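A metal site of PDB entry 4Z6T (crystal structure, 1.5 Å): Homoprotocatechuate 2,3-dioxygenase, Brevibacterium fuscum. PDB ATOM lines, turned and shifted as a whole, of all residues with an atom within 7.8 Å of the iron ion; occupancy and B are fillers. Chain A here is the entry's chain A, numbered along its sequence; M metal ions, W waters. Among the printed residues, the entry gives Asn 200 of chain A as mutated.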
ATOM      1  N   ASP A 154      24.917 -22.477 -21.695  1.00  0.00           N
ATOM      2  CA  ASP A 154      25.287 -21.081 -21.832  1.00  0.00           C
ATOM      3  C   ASP A 154      24.165 -20.055 -21.629  1.00  0.00           C
ATOM      4  O   ASP A 154      24.370 -19.050 -20.904  1.00  0.00           O
ATOM      5  CB  ASP A 154      26.002 -20.765 -23.164  1.00  0.00           C
ATOM      6  CG  ASP A 154      26.618 -19.378 -23.147  1.00  0.00           C
ATOM      7  OD1 ASP A 154      27.652 -19.233 -22.478  1.00  0.00           O
ATOM      8  OD2 ASP A 154      26.035 -18.414 -23.716  1.00  0.00           O
ATOM      9  N   HIS A 155      23.036 -20.257 -22.308  1.00  0.00           N
ATOM     10  CA  HIS A 155      21.965 -19.263 -22.262  1.00  0.00           C
ATOM     11  C   HIS A 155      20.649 -19.762 -22.799  1.00  0.00           C
ATOM     12  O   HIS A 155      20.558 -20.803 -23.396  1.00  0.00           O
ATOM     13  CB  HIS A 155      22.377 -17.974 -23.053  1.00  0.00           C
ATOM     14  CG  HIS A 155      22.526 -18.154 -24.524  1.00  0.00           C
ATOM     15  ND1 HIS A 155      23.744 -18.339 -25.127  1.00  0.00           N
ATOM     16  CD2 HIS A 155      21.617 -18.099 -25.534  1.00  0.00           C
ATOM     17  CE1 HIS A 155      23.588 -18.395 -26.446  1.00  0.00           C
ATOM     18  NE2 HIS A 155      22.301 -18.266 -26.716  1.00  0.00           N
ATOM     19  N   PHE A 156      19.641 -18.945 -22.573  1.00  0.00           N
ATOM     20  CA  PHE A 156      18.332 -19.103 -23.170  1.00  0.00           C
ATOM     21  C   PHE A 156      18.078 -17.912 -24.124  1.00  0.00           C
ATOM     22  O   PHE A 156      18.686 -16.852 -23.985  1.00  0.00           O
ATOM     23  CB  PHE A 156      17.211 -19.056 -22.094  1.00  0.00           C
ATOM     24  CG  PHE A 156      17.449 -19.944 -20.869  1.00  0.00           C
ATOM     25  CD1 PHE A 156      17.682 -21.295 -21.006  1.00  0.00           C
ATOM     26  CD2 PHE A 156      17.393 -19.398 -19.594  1.00  0.00           C
ATOM     27  CE1 PHE A 156      17.829 -22.104 -19.877  1.00  0.00           C
ATOM     28  CE2 PHE A 156      17.570 -20.195 -18.460  1.00  0.00           C
ATOM     29  CZ  PHE A 156      17.794 -21.543 -18.611  1.00  0.00           C
ATOM     30  N   ASN A 157      17.130 -18.080 -25.041  1.00  0.00           N
ATOM     31  CA  ASN A 157      16.676 -16.967 -25.883  1.00  0.00           C
ATOM     32  C   ASN A 157      15.159 -17.056 -26.024  1.00  0.00           C
ATOM     33  O   ASN A 157      14.621 -18.089 -26.429  1.00  0.00           O
ATOM     34  CB  ASN A 157      17.383 -17.036 -27.245  1.00  0.00           C
ATOM     35  CG  ASN A 157      17.127 -15.837 -28.109  1.00  0.00           C
ATOM     36  OD1 ASN A 157      15.985 -15.516 -28.372  1.00  0.00           O
ATOM     37  ND2 ASN A 157      18.182 -15.193 -28.567  1.00  0.00           N
ATOM     38  N   TRP A 192      20.409  -8.842 -25.894  1.00  0.00           N
ATOM     39  CA  TRP A 192      21.080  -9.885 -25.135  1.00  0.00           C
ATOM     40  C   TRP A 192      21.495  -9.320 -23.796  1.00  0.00           C
ATOM     41  O   TRP A 192      21.959  -8.191 -23.721  1.00  0.00           O
ATOM     42  CB  TRP A 192      22.315 -10.324 -25.932  1.00  0.00           C
ATOM     43  CG  TRP A 192      21.995 -11.177 -27.150  1.00  0.00           C
ATOM     44  CD1 TRP A 192      22.065 -12.552 -27.235  1.00  0.00           C
ATOM     45  CD2 TRP A 192      21.524 -10.735 -28.422  1.00  0.00           C
ATOM     46  NE1 TRP A 192      21.678 -12.979 -28.482  1.00  0.00           N
ATOM     47  CE2 TRP A 192      21.350 -11.890 -29.230  1.00  0.00           C
ATOM     48  CE3 TRP A 192      21.273  -9.485 -28.976  1.00  0.00           C
ATOM     49  CZ2 TRP A 192      20.903 -11.812 -30.568  1.00  0.00           C
ATOM     50  CZ3 TRP A 192      20.806  -9.403 -30.293  1.00  0.00           C
ATOM     51  CH2 TRP A 192      20.652 -10.562 -31.087  1.00  0.00           C
ATOM     52  N   ASN A 200      25.429 -13.461 -22.843  1.00  0.00           N
ATOM     53  CA  ASN A 200      24.098 -13.595 -22.275  1.00  0.00           C
ATOM     54  C   ASN A 200      23.842 -14.782 -21.373  1.00  0.00           C
ATOM     55  O   ASN A 200      24.529 -15.795 -21.412  1.00  0.00           O
ATOM     56  CB  ASN A 200      22.965 -13.453 -23.311  1.00  0.00           C
ATOM     57  CG  ASN A 200      22.846 -14.597 -24.245  1.00  0.00           C
ATOM     58  OD1 ASN A 200      23.848 -15.090 -24.768  1.00  0.00           O
ATOM     59  ND2 ASN A 200      21.596 -15.037 -24.490  1.00  0.00           N
ATOM     60  N   ALA A 203      18.055 -13.837 -23.466  1.00  0.00           N
ATOM     61  CA  ALA A 203      18.019 -12.871 -24.555  1.00  0.00           C
ATOM     62  C   ALA A 203      16.589 -12.726 -25.009  1.00  0.00           C
ATOM     63  O   ALA A 203      15.754 -13.597 -24.767  1.00  0.00           O
ATOM     64  CB  ALA A 203      18.921 -13.330 -25.699  1.00  0.00           C
ATOM     65  N   THR A 205      14.239 -11.935 -28.401  1.00  0.00           N
ATOM     66  CA  THR A 205      14.095 -11.877 -29.839  1.00  0.00           C
ATOM     67  C   THR A 205      12.688 -11.374 -30.153  1.00  0.00           C
ATOM     68  O   THR A 205      11.718 -11.952 -29.690  1.00  0.00           O
ATOM     69  CB  THR A 205      14.311 -13.254 -30.491  1.00  0.00           C
ATOM     70  OG1 THR A 205      15.644 -13.712 -30.228  1.00  0.00           O
ATOM     71  CG2 THR A 205      14.080 -13.170 -31.956  1.00  0.00           C
ATOM     72  N   HIS A 213      12.837 -19.338 -27.987  1.00  0.00           N
ATOM     73  CA  HIS A 213      13.547 -19.455 -29.236  1.00  0.00           C
ATOM     74  C   HIS A 213      14.543 -20.604 -29.219  1.00  0.00           C
ATOM     75  O   HIS A 213      14.515 -21.463 -30.120  1.00  0.00           O
ATOM     76  CB  HIS A 213      14.248 -18.150 -29.618  1.00  0.00           C
ATOM     77  CG  HIS A 213      14.624 -18.119 -31.060  1.00  0.00           C
ATOM     78  ND1 HIS A 213      15.743 -18.762 -31.539  1.00  0.00           N
ATOM     79  CD2 HIS A 213      13.990 -17.623 -32.138  1.00  0.00           C
ATOM     80  CE1 HIS A 213      15.790 -18.644 -32.853  1.00  0.00           C
ATOM     81  NE2 HIS A 213      14.741 -17.950 -33.245  1.00  0.00           N
ATOM     82  N   HIS A 214      15.426 -20.618 -28.223  1.00  0.00           N
ATOM     83  CA  HIS A 214      16.362 -21.724 -28.090  1.00  0.00           C
ATOM     84  C   HIS A 214      16.998 -21.813 -26.724  1.00  0.00           C
ATOM     85  O   HIS A 214      16.881 -20.910 -25.907  1.00  0.00           O
ATOM     86  CB  HIS A 214      17.493 -21.649 -29.160  1.00  0.00           C
ATOM     87  CG  HIS A 214      18.300 -20.387 -29.163  1.00  0.00           C
ATOM     88  ND1 HIS A 214      17.993 -19.314 -29.971  1.00  0.00           N
ATOM     89  CD2 HIS A 214      19.401 -20.019 -28.469  1.00  0.00           C
ATOM     90  CE1 HIS A 214      18.893 -18.370 -29.823  1.00  0.00           C
ATOM     91  NE2 HIS A 214      19.760 -18.756 -28.913  1.00  0.00           N
ATOM     92  N   VAL A 215      17.625 -22.980 -26.488  1.00  0.00           N
ATOM     93  CA  VAL A 215      18.551 -23.184 -25.374  1.00  0.00           C
ATOM     94  C   VAL A 215      19.927 -23.400 -25.983  1.00  0.00           C
ATOM     95  O   VAL A 215      20.023 -24.117 -26.999  1.00  0.00           O
ATOM     96  CB  VAL A 215      18.161 -24.429 -24.528  1.00  0.00           C
ATOM     97  CG1 VAL A 215      19.118 -24.600 -23.376  1.00  0.00           C
ATOM     98  CG2 VAL A 215      16.725 -24.253 -24.010  1.00  0.00           C
ATOM     99  N   ALA A 216      20.940 -22.774 -25.402  1.00  0.00           N
ATOM    100  CA  ALA A 216      22.294 -22.861 -25.962  1.00  0.00           C
ATOM    101  C   ALA A 216      23.277 -23.569 -25.017  1.00  0.00           C
ATOM    102  O   ALA A 216      23.336 -23.246 -23.816  1.00  0.00           O
ATOM    103  CB  ALA A 216      22.819 -21.478 -26.283  1.00  0.00           C
ATOM    104  N   HIS A 248      28.846 -15.595 -35.387  1.00  0.00           N
ATOM    105  CA  HIS A 248      27.864 -14.529 -35.081  1.00  0.00           C
ATOM    106  C   HIS A 248      28.532 -13.159 -35.196  1.00  0.00           C
ATOM    107  O   HIS A 248      29.730 -12.982 -34.868  1.00  0.00           O
ATOM    108  CB  HIS A 248      27.332 -14.633 -33.649  1.00  0.00           C
ATOM    109  CG  HIS A 248      26.258 -15.636 -33.462  1.00  0.00           C
ATOM    110  ND1 HIS A 248      25.113 -15.684 -34.237  1.00  0.00           N
ATOM    111  CD2 HIS A 248      26.098 -16.586 -32.510  1.00  0.00           C
ATOM    112  CE1 HIS A 248      24.326 -16.648 -33.796  1.00  0.00           C
ATOM    113  NE2 HIS A 248      24.886 -17.190 -32.747  1.00  0.00           N
ATOM    114  N   VAL A 250      26.595 -10.381 -33.514  1.00  0.00           N
ATOM    115  CA  VAL A 250      26.190 -10.291 -32.111  1.00  0.00           C
ATOM    116  C   VAL A 250      26.780 -11.485 -31.339  1.00  0.00           C
ATOM    117  O   VAL A 250      26.482 -12.627 -31.656  1.00  0.00           O
ATOM    118  CB  VAL A 250      24.659 -10.307 -31.968  1.00  0.00           C
ATOM    119  CG1 VAL A 250      24.267 -10.420 -30.509  1.00  0.00           C
ATOM    120  CG2 VAL A 250      24.019  -9.051 -32.554  1.00  0.00           C
ATOM    121  N   SER A 251      27.597 -11.174 -30.345  1.00  0.00           N
ATOM    122  CA  SER A 251      28.271 -12.132 -29.450  1.00  0.00           C
ATOM    123  C   SER A 251      29.647 -12.544 -29.901  1.00  0.00           C
ATOM    124  O   SER A 251      30.444 -12.964 -29.074  1.00  0.00           O
ATOM    125  CB  SER A 251      27.454 -13.383 -29.112  1.00  0.00           C
ATOM    126  OG  SER A 251      27.569 -14.381 -30.118  1.00  0.00           O
ATOM    127  N   TYR A 255      28.868 -20.714 -33.915  1.00  0.00           N
ATOM    128  CA  TYR A 255      27.510 -21.176 -33.590  1.00  0.00           C
ATOM    129  C   TYR A 255      26.952 -22.169 -34.575  1.00  0.00           C
ATOM    130  O   TYR A 255      27.418 -22.298 -35.730  1.00  0.00           O
ATOM    131  CB  TYR A 255      26.491 -20.007 -33.466  1.00  0.00           C
ATOM    132  CG  TYR A 255      26.102 -19.435 -34.820  1.00  0.00           C
ATOM    133  CD1 TYR A 255      25.031 -19.947 -35.531  1.00  0.00           C
ATOM    134  CD2 TYR A 255      26.819 -18.387 -35.383  1.00  0.00           C
ATOM    135  CE1 TYR A 255      24.681 -19.476 -36.775  1.00  0.00           C
ATOM    136  CE2 TYR A 255      26.484 -17.880 -36.663  1.00  0.00           C
ATOM    137  CZ  TYR A 255      25.428 -18.436 -37.346  1.00  0.00           C
ATOM    138  OH  TYR A 255      25.020 -17.941 -38.581  1.00  0.00           O
ATOM    139  N   LEU A 256      25.897 -22.813 -34.117  1.00  0.00           N
ATOM    140  CA  LEU A 256      25.107 -23.760 -34.914  1.00  0.00           C
ATOM    141  C   LEU A 256      23.717 -23.864 -34.305  1.00  0.00           C
ATOM    142  O   LEU A 256      23.571 -23.852 -33.082  1.00  0.00           O
ATOM    143  CB  LEU A 256      25.773 -25.152 -34.880  1.00  0.00           C
ATOM    144  CG  LEU A 256      25.026 -26.281 -35.564  1.00  0.00           C
ATOM    145  CD1 LEU A 256      25.000 -26.146 -37.087  1.00  0.00           C
ATOM    146  CD2 LEU A 256      25.605 -27.638 -35.185  1.00  0.00           C
ATOM    147  N   TYR A 257      22.688 -23.996 -35.159  1.00  0.00           N
ATOM    148  CA  TYR A 257      21.303 -24.216 -34.678  1.00  0.00           C
ATOM    149  C   TYR A 257      20.790 -25.524 -35.254  1.00  0.00           C
ATOM    150  O   TYR A 257      20.801 -25.720 -36.488  1.00  0.00           O
ATOM    151  CB  TYR A 257      20.356 -23.093 -35.069  1.00  0.00           C
ATOM    152  CG  TYR A 257      20.731 -21.750 -34.478  1.00  0.00           C
ATOM    153  CD1 TYR A 257      20.350 -21.375 -33.183  1.00  0.00           C
ATOM    154  CD2 TYR A 257      21.483 -20.844 -35.224  1.00  0.00           C
ATOM    155  CE1 TYR A 257      20.698 -20.144 -32.662  1.00  0.00           C
ATOM    156  CE2 TYR A 257      21.861 -19.605 -34.685  1.00  0.00           C
ATOM    157  CZ  TYR A 257      21.440 -19.248 -33.426  1.00  0.00           C
ATOM    158  OH  TYR A 257      21.797 -18.030 -32.885  1.00  0.00           O
ATOM    159  N   GLU A 267      20.946 -24.235 -29.727  1.00  0.00           N
ATOM    160  CA  GLU A 267      22.160 -23.640 -30.239  1.00  0.00           C
ATOM    161  C   GLU A 267      23.386 -24.298 -29.613  1.00  0.00           C
ATOM    162  O   GLU A 267      23.433 -24.537 -28.402  1.00  0.00           O
ATOM    163  CB  GLU A 267      22.183 -22.143 -29.926  1.00  0.00           C
ATOM    164  CG  GLU A 267      23.284 -21.392 -30.641  1.00  0.00           C
ATOM    165  CD  GLU A 267      23.344 -19.921 -30.289  1.00  0.00           C
ATOM    166  OE1 GLU A 267      22.589 -19.494 -29.421  1.00  0.00           O
ATOM    167  OE2 GLU A 267      24.160 -19.187 -30.905  1.00  0.00           O
ATOM    168  N   ILE A 268      24.385 -24.546 -30.444  1.00  0.00           N
ATOM    169  CA  ILE A 268      25.734 -24.837 -29.990  1.00  0.00           C
ATOM    170  C   ILE A 268      26.615 -23.622 -30.224  1.00  0.00           C
ATOM    171  O   ILE A 268      26.494 -22.973 -31.266  1.00  0.00           O
ATOM    172  CB  ILE A 268      26.332 -26.094 -30.677  1.00  0.00           C
ATOM    173  CG1 ILE A 268      25.276 -27.186 -30.989  1.00  0.00           C
ATOM    174  CG2 ILE A 268      27.469 -26.657 -29.837  1.00  0.00           C
ATOM    175  CD1 ILE A 268      24.607 -27.739 -29.781  1.00  0.00           C
ATOM    176  N   TYR A 269      27.464 -23.293 -29.254  1.00  0.00           N
ATOM    177  CA  TYR A 269      28.042 -21.963 -29.106  1.00  0.00           C
ATOM    178  C   TYR A 269      29.443 -22.053 -28.531  1.00  0.00           C
ATOM    179  O   TYR A 269      29.699 -22.836 -27.645  1.00  0.00           O
ATOM    180  CB  TYR A 269      27.126 -21.222 -28.138  1.00  0.00           C
ATOM    181  CG  TYR A 269      27.288 -19.765 -27.849  1.00  0.00           C
ATOM    182  CD1 TYR A 269      26.609 -18.810 -28.600  1.00  0.00           C
ATOM    183  CD2 TYR A 269      27.978 -19.348 -26.706  1.00  0.00           C
ATOM    184  CE1 TYR A 269      26.680 -17.466 -28.240  1.00  0.00           C
ATOM    185  CE2 TYR A 269      28.058 -18.013 -26.341  1.00  0.00           C
ATOM    186  CZ  TYR A 269      27.399 -17.071 -27.108  1.00  0.00           C
ATOM    187  OH  TYR A 269      27.437 -15.749 -26.733  1.00  0.00           O
ATOM    188  N   ARG A 293      24.125 -10.992 -37.760  1.00  0.00           N
ATOM    189  CA  ARG A 293      23.720 -12.286 -37.202  1.00  0.00           C
ATOM    190  C   ARG A 293      24.672 -13.391 -37.613  1.00  0.00           C
ATOM    191  O   ARG A 293      25.132 -14.164 -36.794  1.00  0.00           O
ATOM    192  CB  ARG A 293      22.293 -12.613 -37.597  1.00  0.00           C
ATOM    193  CG  ARG A 293      21.259 -11.788 -36.833  1.00  0.00           C
ATOM    194  CD  ARG A 293      19.896 -12.429 -36.831  1.00  0.00           C
ATOM    195  NE  ARG A 293      18.953 -11.705 -35.970  1.00  0.00           N
ATOM    196  CZ  ARG A 293      18.740 -11.888 -34.671  1.00  0.00           C
ATOM    197  NH1 ARG A 293      19.479 -12.724 -33.949  1.00  0.00           N
ATOM    198  NH2 ARG A 293      17.791 -11.196 -34.049  1.00  0.00           N
ATOM    199  N   TRP A 304      14.093 -19.545 -38.879  1.00  0.00           N
ATOM    200  CA  TRP A 304      14.775 -19.071 -37.665  1.00  0.00           C
ATOM    201  C   TRP A 304      13.982 -17.914 -37.054  1.00  0.00           C
ATOM    202  O   TRP A 304      13.951 -17.714 -35.834  1.00  0.00           O
ATOM    203  CB  TRP A 304      16.221 -18.663 -38.006  1.00  0.00           C
ATOM    204  CG  TRP A 304      17.085 -18.570 -36.805  1.00  0.00           C
ATOM    205  CD1 TRP A 304      17.825 -19.587 -36.240  1.00  0.00           C
ATOM    206  CD2 TRP A 304      17.288 -17.421 -35.983  1.00  0.00           C
ATOM    207  NE1 TRP A 304      18.458 -19.133 -35.120  1.00  0.00           N
ATOM    208  CE2 TRP A 304      18.153 -17.799 -34.947  1.00  0.00           C
ATOM    209  CE3 TRP A 304      16.796 -16.115 -36.013  1.00  0.00           C
ATOM    210  CZ2 TRP A 304      18.520 -16.929 -33.941  1.00  0.00           C
ATOM    211  CZ3 TRP A 304      17.173 -15.245 -35.007  1.00  0.00           C
ATOM    212  CH2 TRP A 304      18.026 -15.647 -33.991  1.00  0.00           C
HETATM  213 FE    FE M   1      21.694 -17.672 -28.765  1.00  0.00          FE
HETATM  214  O   HOH W   1      21.369 -16.878 -30.719  1.00  0.00           O
HETATM  215  O   HOH W   2      23.574 -16.609 -29.264  1.00  0.00           O
HETATM  216  O   HOH W   3      20.893 -15.840 -27.892  1.00  0.00           O
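Three residues have an atom within 4 Å of the iron ion: His 155, His 214 and Glu 267.
Water W3 lies within hydrogen-bond range of ND2 of Asn 157 (2.9 Å) and NE1 of Trp 192 (3.0 Å).
ND1 of His 155 sits at hydrogen-bond distance from OD1 of Asn 200, 3.3 Å away. The side-chain hydroxyl (OH) of Tyr 257 sits at hydrogen-bond distance from the side-chain carboxylate (OE2) of Glu 267. The side-chain carboxylate (OD2) of Asp 154 is in hydrogen-bond range of a ring nitrogen (ND1) of His 155 (2.7 Å). A ring nitrogen (NE2) of His 248 is in hydrogen-bond range of the side-chain carboxylate of Glu 267, at 2.8 Å. A ring nitrogen (ND1) of His 213 sits at hydrogen-bond distance from a ring nitrogen (ND1) of His 214 (2.8 Å). The backbone carbonyl oxygen (O) of His 214 lies within hydrogen-bond range of the backbone NH (N) of Asn 157. The backbone NH (N) of Glu 267 sits at hydrogen-bond distance from the backbone carbonyl oxygen (O) of Val 215 (2.9 Å). N of Ala 216 is in hydrogen-bond range of O of His 155 (2.8 Å).
The iron ion is bound by water W1 (2.1 Å), the side-chain carboxylate (OE1) of Glu 267 (2.1 Å), water W3 (2.2 Å), water W2 (2.2 Å), a ring nitrogen (NE2) of His 155 (2.2 Å) and a ring nitrogen (NE2) of His 214 (2.2 Å).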
